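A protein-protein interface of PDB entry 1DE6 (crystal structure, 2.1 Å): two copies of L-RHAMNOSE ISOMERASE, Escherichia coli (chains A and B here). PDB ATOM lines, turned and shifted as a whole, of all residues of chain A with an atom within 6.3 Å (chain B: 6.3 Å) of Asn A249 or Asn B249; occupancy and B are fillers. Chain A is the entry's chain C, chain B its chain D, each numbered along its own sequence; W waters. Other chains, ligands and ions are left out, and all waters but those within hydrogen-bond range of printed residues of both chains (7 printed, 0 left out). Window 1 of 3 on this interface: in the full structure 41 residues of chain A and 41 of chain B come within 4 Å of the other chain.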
ATOM      1  N   SER A 234     -12.118  -4.957  -6.550  1.00  0.00           N
ATOM      2  CA  SER A 234     -11.611  -6.258  -6.108  1.00  0.00           C
ATOM      3  C   SER A 234     -10.217  -6.008  -5.513  1.00  0.00           C
ATOM      4  O   SER A 234      -9.546  -4.958  -5.674  1.00  0.00           O
ATOM      5  CB  SER A 234     -11.366  -7.244  -7.238  1.00  0.00           C
ATOM      6  OG  SER A 234     -10.332  -6.804  -8.154  1.00  0.00           O
ATOM      7  N   LYS A 235      -9.788  -7.041  -4.833  1.00  0.00           N
ATOM      8  CA  LYS A 235      -8.499  -7.114  -4.199  1.00  0.00           C
ATOM      9  C   LYS A 235      -8.162  -8.578  -4.053  1.00  0.00           C
ATOM     10  O   LYS A 235      -9.082  -9.383  -3.733  1.00  0.00           O
ATOM     11  CB  LYS A 235      -8.429  -6.435  -2.840  1.00  0.00           C
ATOM     12  CG  LYS A 235      -7.015  -6.287  -2.386  1.00  0.00           C
ATOM     13  CD  LYS A 235      -6.940  -5.552  -1.071  1.00  0.00           C
ATOM     14  CE  LYS A 235      -5.526  -5.213  -0.668  1.00  0.00           C
ATOM     15  NZ  LYS A 235      -5.643  -4.319   0.496  1.00  0.00           N
ATOM     16  N   LEU A 236      -6.849  -8.875  -4.268  1.00  0.00           N
ATOM     17  CA  LEU A 236      -6.397 -10.287  -4.118  1.00  0.00           C
ATOM     18  C   LEU A 236      -6.177 -10.733  -2.682  1.00  0.00           C
ATOM     19  O   LEU A 236      -6.563 -11.806  -2.178  1.00  0.00           O
ATOM     20  CB  LEU A 236      -5.222 -10.684  -5.025  1.00  0.00           C
ATOM     21  CG  LEU A 236      -4.731 -12.109  -4.788  1.00  0.00           C
ATOM     22  CD1 LEU A 236      -5.758 -13.083  -5.344  1.00  0.00           C
ATOM     23  CD2 LEU A 236      -3.395 -12.326  -5.531  1.00  0.00           C
ATOM     24  N   GLY A 247     -14.561 -10.128  -1.864  1.00  0.00           N
ATOM     25  CA  GLY A 247     -14.727  -9.448  -3.111  1.00  0.00           C
ATOM     26  C   GLY A 247     -13.524  -9.544  -4.015  1.00  0.00           C
ATOM     27  O   GLY A 247     -12.650  -8.653  -4.097  1.00  0.00           O
ATOM     28  N   SER A 248     -13.491 -10.683  -4.680  1.00  0.00           N
ATOM     29  CA  SER A 248     -12.433 -11.034  -5.613  1.00  0.00           C
ATOM     30  C   SER A 248     -12.599 -10.399  -6.993  1.00  0.00           C
ATOM     31  O   SER A 248     -13.566  -9.691  -7.310  1.00  0.00           O
ATOM     32  CB  SER A 248     -12.327 -12.547  -5.618  1.00  0.00           C
ATOM     33  OG  SER A 248     -13.558 -12.919  -6.229  1.00  0.00           O
ATOM     34  N   ASN A 249     -11.595 -10.607  -7.854  1.00  0.00           N
ATOM     35  CA  ASN A 249     -11.683 -10.025  -9.159  1.00  0.00           C
ATOM     36  C   ASN A 249     -12.967 -10.507  -9.876  1.00  0.00           C
ATOM     37  O   ASN A 249     -13.810  -9.719 -10.414  1.00  0.00           O
ATOM     38  CB  ASN A 249     -10.481 -10.599  -9.934  1.00  0.00           C
ATOM     39  CG  ASN A 249     -10.509 -10.475 -11.444  1.00  0.00           C
ATOM     40  OD1 ASN A 249     -11.368  -9.855 -12.067  1.00  0.00           O
ATOM     41  ND2 ASN A 249      -9.421 -10.912 -12.071  1.00  0.00           N
ATOM     42  N   GLU A 250     -13.104 -11.853  -9.940  1.00  0.00           N
ATOM     43  CA  GLU A 250     -14.271 -12.427 -10.630  1.00  0.00           C
ATOM     44  C   GLU A 250     -15.604 -11.956 -10.054  1.00  0.00           C
ATOM     45  O   GLU A 250     -16.603 -11.727 -10.770  1.00  0.00           O
ATOM     46  CB  GLU A 250     -14.174 -13.948 -10.678  1.00  0.00           C
ATOM     47  CG  GLU A 250     -12.968 -14.279 -11.550  1.00  0.00           C
ATOM     48  CD  GLU A 250     -11.640 -14.273 -10.820  1.00  0.00           C
ATOM     49  OE1 GLU A 250     -11.477 -14.154  -9.617  1.00  0.00           O
ATOM     50  OE2 GLU A 250     -10.669 -14.487 -11.629  1.00  0.00           O
ATOM     51  N   PHE A 251     -15.582 -11.850  -8.733  1.00  0.00           N
ATOM     52  CA  PHE A 251     -16.779 -11.409  -8.001  1.00  0.00           C
ATOM     53  C   PHE A 251     -17.292 -10.053  -8.483  1.00  0.00           C
ATOM     54  O   PHE A 251     -18.491  -9.836  -8.813  1.00  0.00           O
ATOM     55  CB  PHE A 251     -16.567 -11.438  -6.485  1.00  0.00           C
ATOM     56  CG  PHE A 251     -17.805 -10.988  -5.776  1.00  0.00           C
ATOM     57  CD1 PHE A 251     -18.774 -11.888  -5.333  1.00  0.00           C
ATOM     58  CD2 PHE A 251     -18.039  -9.627  -5.608  1.00  0.00           C
ATOM     59  CE1 PHE A 251     -19.979 -11.476  -4.744  1.00  0.00           C
ATOM     60  CE2 PHE A 251     -19.195  -9.204  -4.962  1.00  0.00           C
ATOM     61  CZ  PHE A 251     -20.181 -10.113  -4.561  1.00  0.00           C
ATOM     62  N   TYR A 252     -16.363  -9.119  -8.570  1.00  0.00           N
ATOM     63  CA  TYR A 252     -16.777  -7.799  -8.996  1.00  0.00           C
ATOM     64  C   TYR A 252     -16.934  -7.695 -10.455  1.00  0.00           C
ATOM     65  O   TYR A 252     -17.663  -6.832 -10.988  1.00  0.00           O
ATOM     66  CB  TYR A 252     -15.689  -6.844  -8.533  1.00  0.00           C
ATOM     67  CG  TYR A 252     -15.877  -6.629  -7.059  1.00  0.00           C
ATOM     68  CD1 TYR A 252     -17.139  -6.344  -6.550  1.00  0.00           C
ATOM     69  CD2 TYR A 252     -14.805  -6.611  -6.168  1.00  0.00           C
ATOM     70  CE1 TYR A 252     -17.368  -6.031  -5.202  1.00  0.00           C
ATOM     71  CE2 TYR A 252     -14.997  -6.316  -4.820  1.00  0.00           C
ATOM     72  CZ  TYR A 252     -16.287  -6.062  -4.331  1.00  0.00           C
ATOM     73  OH  TYR A 252     -16.481  -5.699  -3.037  1.00  0.00           O
ATOM     74  N   MET A 253     -16.173  -8.539 -11.123  1.00  0.00           N
ATOM     75  CA  MET A 253     -16.297  -8.500 -12.556  1.00  0.00           C
ATOM     76  C   MET A 253     -17.744  -8.922 -12.863  1.00  0.00           C
ATOM     77  O   MET A 253     -18.502  -8.268 -13.646  1.00  0.00           O
ATOM     78  CB  MET A 253     -15.258  -9.369 -13.290  1.00  0.00           C
ATOM     79  CG  MET A 253     -15.548  -9.356 -14.774  1.00  0.00           C
ATOM     80  SD  MET A 253     -15.112  -7.760 -15.534  1.00  0.00           S
ATOM     81  CE  MET A 253     -15.823  -7.868 -17.211  1.00  0.00           C
ATOM     82  N   GLY A 254     -18.144 -10.016 -12.217  1.00  0.00           N
ATOM     83  CA  GLY A 254     -19.539 -10.424 -12.470  1.00  0.00           C
ATOM     84  C   GLY A 254     -20.475  -9.333 -12.041  1.00  0.00           C
ATOM     85  O   GLY A 254     -21.318  -8.954 -12.791  1.00  0.00           O
ATOM     86  N   LEU A 263     -16.394  -0.423 -12.716  1.00  0.00           N
ATOM     87  CA  LEU A 263     -15.478  -1.403 -12.137  1.00  0.00           C
ATOM     88  C   LEU A 263     -14.154  -0.683 -11.912  1.00  0.00           C
ATOM     89  O   LEU A 263     -13.618   0.050 -12.785  1.00  0.00           O
ATOM     90  CB  LEU A 263     -15.243  -2.646 -13.027  1.00  0.00           C
ATOM     91  CG  LEU A 263     -14.227  -3.651 -12.515  1.00  0.00           C
ATOM     92  CD1 LEU A 263     -14.838  -4.574 -11.448  1.00  0.00           C
ATOM     93  CD2 LEU A 263     -13.870  -4.533 -13.667  1.00  0.00           C
ATOM     94  N   LEU A 265     -10.304  -0.933 -11.173  1.00  0.00           N
ATOM     95  CA  LEU A 265      -9.144  -1.858 -11.319  1.00  0.00           C
ATOM     96  C   LEU A 265      -7.977  -1.174 -10.650  1.00  0.00           C
ATOM     97  O   LEU A 265      -7.627  -0.044 -11.041  1.00  0.00           O
ATOM     98  CB  LEU A 265      -8.789  -2.090 -12.806  1.00  0.00           C
ATOM     99  CG  LEU A 265      -9.885  -2.707 -13.601  1.00  0.00           C
ATOM    100  CD1 LEU A 265      -9.549  -2.637 -15.081  1.00  0.00           C
ATOM    101  CD2 LEU A 265      -9.949  -4.159 -13.146  1.00  0.00           C
ATOM    102  N   PHE A 270      -3.646  -7.372  -7.705  1.00  0.00           N
ATOM    103  CA  PHE A 270      -3.667  -8.625  -8.423  1.00  0.00           C
ATOM    104  C   PHE A 270      -2.489  -9.587  -8.088  1.00  0.00           C
ATOM    105  O   PHE A 270      -1.730  -9.328  -7.147  1.00  0.00           O
ATOM    106  CB  PHE A 270      -3.795  -8.280  -9.890  1.00  0.00           C
ATOM    107  CG  PHE A 270      -5.142  -7.695 -10.090  1.00  0.00           C
ATOM    108  CD1 PHE A 270      -5.354  -6.333  -9.909  1.00  0.00           C
ATOM    109  CD2 PHE A 270      -6.239  -8.513 -10.394  1.00  0.00           C
ATOM    110  CE1 PHE A 270      -6.644  -5.806 -10.094  1.00  0.00           C
ATOM    111  CE2 PHE A 270      -7.529  -8.011 -10.618  1.00  0.00           C
ATOM    112  CZ  PHE A 270      -7.723  -6.625 -10.477  1.00  0.00           C
ATOM    113  N   HIS A 271      -2.380 -10.687  -8.828  1.00  0.00           N
ATOM    114  CA  HIS A 271      -1.352 -11.679  -8.619  1.00  0.00           C
ATOM    115  C   HIS A 271      -0.023 -11.180  -9.152  1.00  0.00           C
ATOM    116  O   HIS A 271       0.052 -10.239  -9.890  1.00  0.00           O
ATOM    117  CB  HIS A 271      -1.737 -12.957  -9.431  1.00  0.00           C
ATOM    118  CG  HIS A 271      -3.025 -13.571  -8.949  1.00  0.00           C
ATOM    119  ND1 HIS A 271      -4.321 -13.285  -9.283  1.00  0.00           N
ATOM    120  CD2 HIS A 271      -3.019 -14.531  -7.947  1.00  0.00           C
ATOM    121  CE1 HIS A 271      -5.102 -14.113  -8.468  1.00  0.00           C
ATOM    122  NE2 HIS A 271      -4.307 -14.859  -7.714  1.00  0.00           N
ATOM    123  N   GLU A 274       0.570  -9.979 -12.785  1.00  0.00           N
ATOM    124  CA  GLU A 274      -0.748  -9.642 -13.358  1.00  0.00           C
ATOM    125  C   GLU A 274      -0.863  -8.140 -13.569  1.00  0.00           C
ATOM    126  O   GLU A 274      -0.513  -7.415 -12.648  1.00  0.00           O
ATOM    127  CB  GLU A 274      -1.869 -10.026 -12.412  1.00  0.00           C
ATOM    128  CG  GLU A 274      -3.247  -9.898 -13.138  1.00  0.00           C
ATOM    129  CD  GLU A 274      -4.253 -10.710 -12.385  1.00  0.00           C
ATOM    130  OE1 GLU A 274      -4.026 -11.080 -11.266  1.00  0.00           O
ATOM    131  OE2 GLU A 274      -5.348 -10.978 -13.013  1.00  0.00           O
ATOM    132  N   ASP A 278      -3.894  -4.772 -19.210  1.00  0.00           N
ATOM    133  CA  ASP A 278      -4.447  -5.754 -20.133  1.00  0.00           C
ATOM    134  C   ASP A 278      -5.947  -5.854 -19.900  1.00  0.00           C
ATOM    135  O   ASP A 278      -6.730  -6.028 -20.831  1.00  0.00           O
ATOM    136  CB  ASP A 278      -3.880  -7.130 -19.806  1.00  0.00           C
ATOM    137  CG  ASP A 278      -4.688  -8.248 -20.532  1.00  0.00           C
ATOM    138  OD1 ASP A 278      -4.682  -8.452 -21.774  1.00  0.00           O
ATOM    139  OD2 ASP A 278      -5.462  -8.965 -19.717  1.00  0.00           O
ATOM    140  N   LYS A 279      -6.358  -5.707 -18.646  1.00  0.00           N
ATOM    141  CA  LYS A 279      -7.789  -5.787 -18.360  1.00  0.00           C
ATOM    142  C   LYS A 279      -8.684  -4.644 -18.851  1.00  0.00           C
ATOM    143  O   LYS A 279      -9.864  -4.807 -18.960  1.00  0.00           O
ATOM    144  CB  LYS A 279      -7.978  -5.913 -16.887  1.00  0.00           C
ATOM    145  CG  LYS A 279      -7.121  -7.049 -16.361  1.00  0.00           C
ATOM    146  CD  LYS A 279      -7.158  -7.065 -14.866  1.00  0.00           C
ATOM    147  CE  LYS A 279      -6.255  -8.114 -14.165  1.00  0.00           C
ATOM    148  NZ  LYS A 279      -6.324  -9.453 -14.790  1.00  0.00           N
ATOM    149  N   SER B 234     -11.156 -19.029 -20.767  1.00  0.00           N
ATOM    150  CA  SER B 234     -10.104 -18.036 -20.792  1.00  0.00           C
ATOM    151  C   SER B 234      -8.777 -18.779 -20.700  1.00  0.00           C
ATOM    152  O   SER B 234      -8.688 -20.003 -20.304  1.00  0.00           O
ATOM    153  CB  SER B 234     -10.153 -16.994 -19.669  1.00  0.00           C
ATOM    154  OG  SER B 234      -9.822 -17.577 -18.383  1.00  0.00           O
ATOM    155  N   LYS B 235      -7.761 -17.968 -21.039  1.00  0.00           N
ATOM    156  CA  LYS B 235      -6.339 -18.374 -20.990  1.00  0.00           C
ATOM    157  C   LYS B 235      -5.458 -17.166 -20.848  1.00  0.00           C
ATOM    158  O   LYS B 235      -5.740 -16.132 -21.509  1.00  0.00           O
ATOM    159  CB  LYS B 235      -5.919 -19.084 -22.271  1.00  0.00           C
ATOM    160  CG  LYS B 235      -4.674 -19.931 -22.031  1.00  0.00           C
ATOM    161  CD  LYS B 235      -4.366 -20.916 -23.146  1.00  0.00           C
ATOM    162  CE  LYS B 235      -3.033 -21.611 -22.926  1.00  0.00           C
ATOM    163  NZ  LYS B 235      -2.624 -22.411 -24.084  1.00  0.00           N
ATOM    164  N   LEU B 236      -4.391 -17.315 -20.038  1.00  0.00           N
ATOM    165  CA  LEU B 236      -3.486 -16.204 -19.800  1.00  0.00           C
ATOM    166  C   LEU B 236      -2.554 -15.935 -20.956  1.00  0.00           C
ATOM    167  O   LEU B 236      -2.508 -14.858 -21.584  1.00  0.00           O
ATOM    168  CB  LEU B 236      -2.693 -16.320 -18.527  1.00  0.00           C
ATOM    169  CG  LEU B 236      -1.813 -15.075 -18.353  1.00  0.00           C
ATOM    170  CD1 LEU B 236      -2.656 -13.798 -18.242  1.00  0.00           C
ATOM    171  CD2 LEU B 236      -1.007 -15.281 -17.080  1.00  0.00           C
ATOM    172  N   GLY B 247      -9.131 -13.708 -25.590  1.00  0.00           N
ATOM    173  CA  GLY B 247     -10.055 -14.292 -24.643  1.00  0.00           C
ATOM    174  C   GLY B 247      -9.392 -14.502 -23.289  1.00  0.00           C
ATOM    175  O   GLY B 247      -9.021 -15.628 -22.892  1.00  0.00           O
ATOM    176  N   SER B 248      -9.282 -13.396 -22.549  1.00  0.00           N
ATOM    177  CA  SER B 248      -8.719 -13.333 -21.209  1.00  0.00           C
ATOM    178  C   SER B 248      -9.799 -13.642 -20.152  1.00  0.00           C
ATOM    179  O   SER B 248     -10.974 -13.784 -20.443  1.00  0.00           O
ATOM    180  CB  SER B 248      -8.240 -11.930 -20.962  1.00  0.00           C
ATOM    181  OG  SER B 248      -9.388 -11.044 -21.056  1.00  0.00           O
ATOM    182  N   ASN B 249      -9.366 -13.750 -18.912  1.00  0.00           N
ATOM    183  CA  ASN B 249     -10.189 -14.053 -17.819  1.00  0.00           C
ATOM    184  C   ASN B 249     -11.362 -13.087 -17.752  1.00  0.00           C
ATOM    185  O   ASN B 249     -12.540 -13.520 -17.712  1.00  0.00           O
ATOM    186  CB  ASN B 249      -9.316 -14.013 -16.571  1.00  0.00           C
ATOM    187  CG  ASN B 249     -10.097 -13.943 -15.275  1.00  0.00           C
ATOM    188  OD1 ASN B 249     -11.299 -14.197 -15.247  1.00  0.00           O
ATOM    189  ND2 ASN B 249      -9.416 -13.778 -14.145  1.00  0.00           N
ATOM    190  N   GLU B 250     -11.076 -11.819 -17.696  1.00  0.00           N
ATOM    191  CA  GLU B 250     -12.146 -10.803 -17.570  1.00  0.00           C
ATOM    192  C   GLU B 250     -13.139 -10.836 -18.715  1.00  0.00           C
ATOM    193  O   GLU B 250     -14.349 -10.736 -18.563  1.00  0.00           O
ATOM    194  CB  GLU B 250     -11.536  -9.380 -17.409  1.00  0.00           C
ATOM    195  CG  GLU B 250     -10.843  -9.230 -16.051  1.00  0.00           C
ATOM    196  CD  GLU B 250      -9.496  -9.898 -15.979  1.00  0.00           C
ATOM    197  OE1 GLU B 250      -8.876 -10.251 -16.954  1.00  0.00           O
ATOM    198  OE2 GLU B 250      -9.070 -10.026 -14.758  1.00  0.00           O
ATOM    199  N   PHE B 251     -12.582 -10.971 -19.892  1.00  0.00           N
ATOM    200  CA  PHE B 251     -13.347 -11.026 -21.115  1.00  0.00           C
ATOM    201  C   PHE B 251     -14.477 -12.105 -21.084  1.00  0.00           C
ATOM    202  O   PHE B 251     -15.608 -11.886 -21.509  1.00  0.00           O
ATOM    203  CB  PHE B 251     -12.397 -11.216 -22.325  1.00  0.00           C
ATOM    204  CG  PHE B 251     -13.223 -11.408 -23.559  1.00  0.00           C
ATOM    205  CD1 PHE B 251     -13.540 -10.293 -24.326  1.00  0.00           C
ATOM    206  CD2 PHE B 251     -13.768 -12.642 -23.937  1.00  0.00           C
ATOM    207  CE1 PHE B 251     -14.327 -10.400 -25.476  1.00  0.00           C
ATOM    208  CE2 PHE B 251     -14.550 -12.772 -25.090  1.00  0.00           C
ATOM    209  CZ  PHE B 251     -14.820 -11.643 -25.871  1.00  0.00           C
ATOM    210  N   TYR B 252     -14.135 -13.285 -20.600  1.00  0.00           N
ATOM    211  CA  TYR B 252     -15.000 -14.443 -20.533  1.00  0.00           C
ATOM    212  C   TYR B 252     -15.861 -14.440 -19.304  1.00  0.00           C
ATOM    213  O   TYR B 252     -16.975 -15.034 -19.256  1.00  0.00           O
ATOM    214  CB  TYR B 252     -14.242 -15.774 -20.648  1.00  0.00           C
ATOM    215  CG  TYR B 252     -13.843 -16.077 -22.034  1.00  0.00           C
ATOM    216  CD1 TYR B 252     -14.742 -15.914 -23.093  1.00  0.00           C
ATOM    217  CD2 TYR B 252     -12.546 -16.511 -22.321  1.00  0.00           C
ATOM    218  CE1 TYR B 252     -14.397 -16.279 -24.405  1.00  0.00           C
ATOM    219  CE2 TYR B 252     -12.176 -16.842 -23.632  1.00  0.00           C
ATOM    220  CZ  TYR B 252     -13.107 -16.768 -24.675  1.00  0.00           C
ATOM    221  OH  TYR B 252     -12.749 -17.129 -25.956  1.00  0.00           O
ATOM    222  N   MET B 253     -15.315 -13.781 -18.286  1.00  0.00           N
ATOM    223  CA  MET B 253     -16.116 -13.600 -17.078  1.00  0.00           C
ATOM    224  C   MET B 253     -17.263 -12.648 -17.487  1.00  0.00           C
ATOM    225  O   MET B 253     -18.446 -12.841 -17.235  1.00  0.00           O
ATOM    226  CB  MET B 253     -15.340 -12.997 -15.893  1.00  0.00           C
ATOM    227  CG  MET B 253     -16.266 -12.879 -14.695  1.00  0.00           C
ATOM    228  SD  MET B 253     -16.853 -14.453 -13.965  1.00  0.00           S
ATOM    229  CE  MET B 253     -18.126 -13.869 -12.803  1.00  0.00           C
ATOM    230  N   GLY B 254     -16.888 -11.622 -18.232  1.00  0.00           N
ATOM    231  CA  GLY B 254     -17.871 -10.703 -18.673  1.00  0.00           C
ATOM    232  C   GLY B 254     -18.862 -11.408 -19.556  1.00  0.00           C
ATOM    233  O   GLY B 254     -20.096 -11.317 -19.367  1.00  0.00           O
ATOM    234  N   LEU B 263     -19.130 -21.062 -17.784  1.00  0.00           N
ATOM    235  CA  LEU B 263     -17.787 -20.546 -17.791  1.00  0.00           C
ATOM    236  C   LEU B 263     -16.837 -21.661 -17.519  1.00  0.00           C
ATOM    237  O   LEU B 263     -17.045 -22.426 -16.593  1.00  0.00           O
ATOM    238  CB  LEU B 263     -17.593 -19.403 -16.726  1.00  0.00           C
ATOM    239  CG  LEU B 263     -16.140 -18.845 -16.603  1.00  0.00           C
ATOM    240  CD1 LEU B 263     -15.815 -17.919 -17.755  1.00  0.00           C
ATOM    241  CD2 LEU B 263     -16.074 -18.019 -15.338  1.00  0.00           C
ATOM    242  N   LEU B 265     -13.225 -22.842 -16.327  1.00  0.00           N
ATOM    243  CA  LEU B 265     -12.070 -22.508 -15.534  1.00  0.00           C
ATOM    244  C   LEU B 265     -11.061 -23.635 -15.609  1.00  0.00           C
ATOM    245  O   LEU B 265     -11.284 -24.705 -15.117  1.00  0.00           O
ATOM    246  CB  LEU B 265     -12.370 -22.221 -14.037  1.00  0.00           C
ATOM    247  CG  LEU B 265     -13.422 -21.109 -13.747  1.00  0.00           C
ATOM    248  CD1 LEU B 265     -13.865 -21.076 -12.234  1.00  0.00           C
ATOM    249  CD2 LEU B 265     -12.922 -19.704 -14.230  1.00  0.00           C
ATOM    250  N   PHE B 270      -3.895 -19.562 -15.624  1.00  0.00           N
ATOM    251  CA  PHE B 270      -3.853 -18.340 -14.838  1.00  0.00           C
ATOM    252  C   PHE B 270      -2.468 -17.868 -14.488  1.00  0.00           C
ATOM    253  O   PHE B 270      -1.517 -18.440 -15.006  1.00  0.00           O
ATOM    254  CB  PHE B 270      -4.728 -18.584 -13.580  1.00  0.00           C
ATOM    255  CG  PHE B 270      -6.164 -18.624 -14.086  1.00  0.00           C
ATOM    256  CD1 PHE B 270      -6.732 -19.830 -14.503  1.00  0.00           C
ATOM    257  CD2 PHE B 270      -6.871 -17.439 -14.304  1.00  0.00           C
ATOM    258  CE1 PHE B 270      -8.025 -19.861 -15.042  1.00  0.00           C
ATOM    259  CE2 PHE B 270      -8.164 -17.445 -14.835  1.00  0.00           C
ATOM    260  CZ  PHE B 270      -8.755 -18.667 -15.185  1.00  0.00           C
ATOM    261  N   HIS B 271      -2.406 -16.824 -13.648  1.00  0.00           N
ATOM    262  CA  HIS B 271      -1.175 -16.244 -13.216  1.00  0.00           C
ATOM    263  C   HIS B 271      -0.455 -17.129 -12.212  1.00  0.00           C
ATOM    264  O   HIS B 271      -1.004 -18.086 -11.713  1.00  0.00           O
ATOM    265  CB  HIS B 271      -1.394 -14.836 -12.630  1.00  0.00           C
ATOM    266  CG  HIS B 271      -1.936 -13.857 -13.628  1.00  0.00           C
ATOM    267  ND1 HIS B 271      -3.186 -13.744 -14.135  1.00  0.00           N
ATOM    268  CD2 HIS B 271      -1.111 -12.888 -14.232  1.00  0.00           C
ATOM    269  CE1 HIS B 271      -3.130 -12.676 -15.034  1.00  0.00           C
ATOM    270  NE2 HIS B 271      -1.881 -12.216 -15.082  1.00  0.00           N
ATOM    271  N   GLU B 274      -2.049 -18.017  -8.934  1.00  0.00           N
ATOM    272  CA  GLU B 274      -3.490 -17.841  -9.077  1.00  0.00           C
ATOM    273  C   GLU B 274      -4.200 -19.185  -9.067  1.00  0.00           C
ATOM    274  O   GLU B 274      -3.715 -20.052  -9.761  1.00  0.00           O
ATOM    275  CB  GLU B 274      -3.803 -17.310 -10.416  1.00  0.00           C
ATOM    276  CG  GLU B 274      -5.276 -16.874 -10.479  1.00  0.00           C
ATOM    277  CD  GLU B 274      -5.378 -15.763 -11.508  1.00  0.00           C
ATOM    278  OE1 GLU B 274      -4.501 -15.546 -12.363  1.00  0.00           O
ATOM    279  OE2 GLU B 274      -6.493 -15.071 -11.435  1.00  0.00           O
ATOM    280  N   ASP B 278     -10.392 -20.795  -5.708  1.00  0.00           N
ATOM    281  CA  ASP B 278     -10.977 -19.626  -5.136  1.00  0.00           C
ATOM    282  C   ASP B 278     -12.121 -19.115  -6.056  1.00  0.00           C
ATOM    283  O   ASP B 278     -13.152 -18.588  -5.584  1.00  0.00           O
ATOM    284  CB  ASP B 278      -9.927 -18.449  -4.965  1.00  0.00           C
ATOM    285  CG  ASP B 278     -10.548 -17.063  -4.735  1.00  0.00           C
ATOM    286  OD1 ASP B 278     -11.050 -16.729  -3.653  1.00  0.00           O
ATOM    287  OD2 ASP B 278     -10.562 -16.257  -5.779  1.00  0.00           O
ATOM    288  N   LYS B 279     -11.956 -19.231  -7.378  1.00  0.00           N
ATOM    289  CA  LYS B 279     -12.933 -18.659  -8.299  1.00  0.00           C
ATOM    290  C   LYS B 279     -14.286 -19.321  -8.361  1.00  0.00           C
ATOM    291  O   LYS B 279     -15.281 -18.678  -8.736  1.00  0.00           O
ATOM    292  CB  LYS B 279     -12.417 -18.449  -9.730  1.00  0.00           C
ATOM    293  CG  LYS B 279     -11.052 -17.801  -9.723  1.00  0.00           C
ATOM    294  CD  LYS B 279     -10.214 -18.002 -10.989  1.00  0.00           C
ATOM    295  CE  LYS B 279      -8.800 -17.397 -10.901  1.00  0.00           C
ATOM    296  NZ  LYS B 279      -8.737 -15.955 -10.473  1.00  0.00           N
HETATM  297  O   HOH W   1     -12.556 -15.189  -7.322  1.00  0.00           O
HETATM  298  O   HOH W   2     -12.800 -11.633 -14.207  1.00  0.00           O
HETATM  299  O   HOH W   3      -7.146 -12.173 -11.146  1.00  0.00           O
HETATM  300  O   HOH W   4      -8.403  -9.149 -19.367  1.00  0.00           O
HETATM  301  O   HOH W   5      -6.653 -13.424 -14.086  1.00  0.00           O
HETATM  302  O   HOH W   6      -8.879 -13.818  -8.937  1.00  0.00           O
HETATM  303  O   HOH W   7      -6.496 -11.825 -16.658  1.00  0.00           O
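The side-chain amide nitrogen (ND2) of Asn A249 sits at hydrogen-bond distance from the side-chain carboxylate (OE2) of Glu B250 (2.9 Å). OE2 of Glu A250 lies within hydrogen-bond range of ND2 of Asn B249 (2.9 Å). The side-chain amino group (NZ) of Lys B279 is in salt-bridge range of the side-chain carboxylate (OE2) of Glu A250 (2.7 Å). NZ of Lys A279 lies within salt-bridge range of OE2 of Glu B250.
The side-chain carboxylate of Glu A274 sits at hydrogen-bond distance from the backbone NH of His A271, 3.0 Å away. OE2 of Glu A274 lies within salt-bridge range of NZ of Lys A279, 2.5 Å away. The backbone NH of His B271 sits at hydrogen-bond distance from the side-chain carboxylate of Glu B274 (2.8 Å). The side-chain carboxylate (OE2) of Glu B274 is in salt-bridge range of the side-chain amino group (NZ) of Lys B279, 2.6 Å away.
Among the printed residues, pairs that only touch across the chains: Glu A274 with His B271 (3.3 Å), Glu A250 with Met B253 (3.3 Å), His A271 with Glu B274 (3.4 Å), Met A253 with Glu B250 (3.5 Å), Asn A249 with Asn B249 (3.5 Å), Met A253 with Met B253 (3.6 Å), His A271 with His B271 (3.7 Å), Gly A254 with Met B253 (3.7 Å) and Met A253 with Gly B254 (3.8 Å).
Asn A249 touches just these residues of chain B: Asn B249 and Glu B250. Asn B249 touches two residues of chain A. Of the printed residues of chain A, Glu B274 touches His A271 (3.4 Å). Of the printed residues of chain A, Glu B250 touches Asn A249, Met A253 and Lys A279. Printed residues of chain A within 4 Å of Met B253: Glu A250, Met A253 and Gly A254.
Printed residues of chain B that touch a printed residue of chain A: Asn B249, Glu B250, Met B253, Gly B254, His B271, Glu B274 and Lys B279. Hydrophobic or aromatic side chains of chain B within 4 Å of the printed part of chain A: Met B253 and His B271. Hydrophobic or aromatic side chains of chain A within 4 Å of the printed part of chain B: Met A253 and His A271.
Asn A249 touches Glu B250, and with the chains exchanged Glu A250 touches Asn B249. Glu A250 touches Met B253, and with the chains exchanged Met A253 touches Glu B250. Met B253 touches its own counterpart, Met A253. His B271 touches its own counterpart, His A271. 18 positions are printed for both chains.
Water W6 lies within hydrogen-bond range of NZ of Lys B279 (2.6 Å) and OE1 of Glu A250 (2.7 Å). Water W4 lies within hydrogen-bond range of the side-chain carboxylate (OE1) of Glu B250, the side-chain hydroxyl (OG) of Ser B248 and the side-chain carboxylate (OD2) of Asp A278. Water W3 lies within hydrogen-bond range of ND2 of Asn A249 (2.8 Å), OE2 of Glu A274 (2.9 Å) and OE2 of Glu B274 (3.0 Å). Water W5 lies within hydrogen-bond range of ND2 of Asn B249, OE2 of Glu A274, OE2 of Glu B274 and ND1 of His B271. Water W7 bridges the side-chain carboxylate of Glu B250 and the side-chain amino group of Lys A279. Water W2 bridges the side-chain amide oxygen of Asn A249 and the side-chain amide oxygen of Asn B249.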
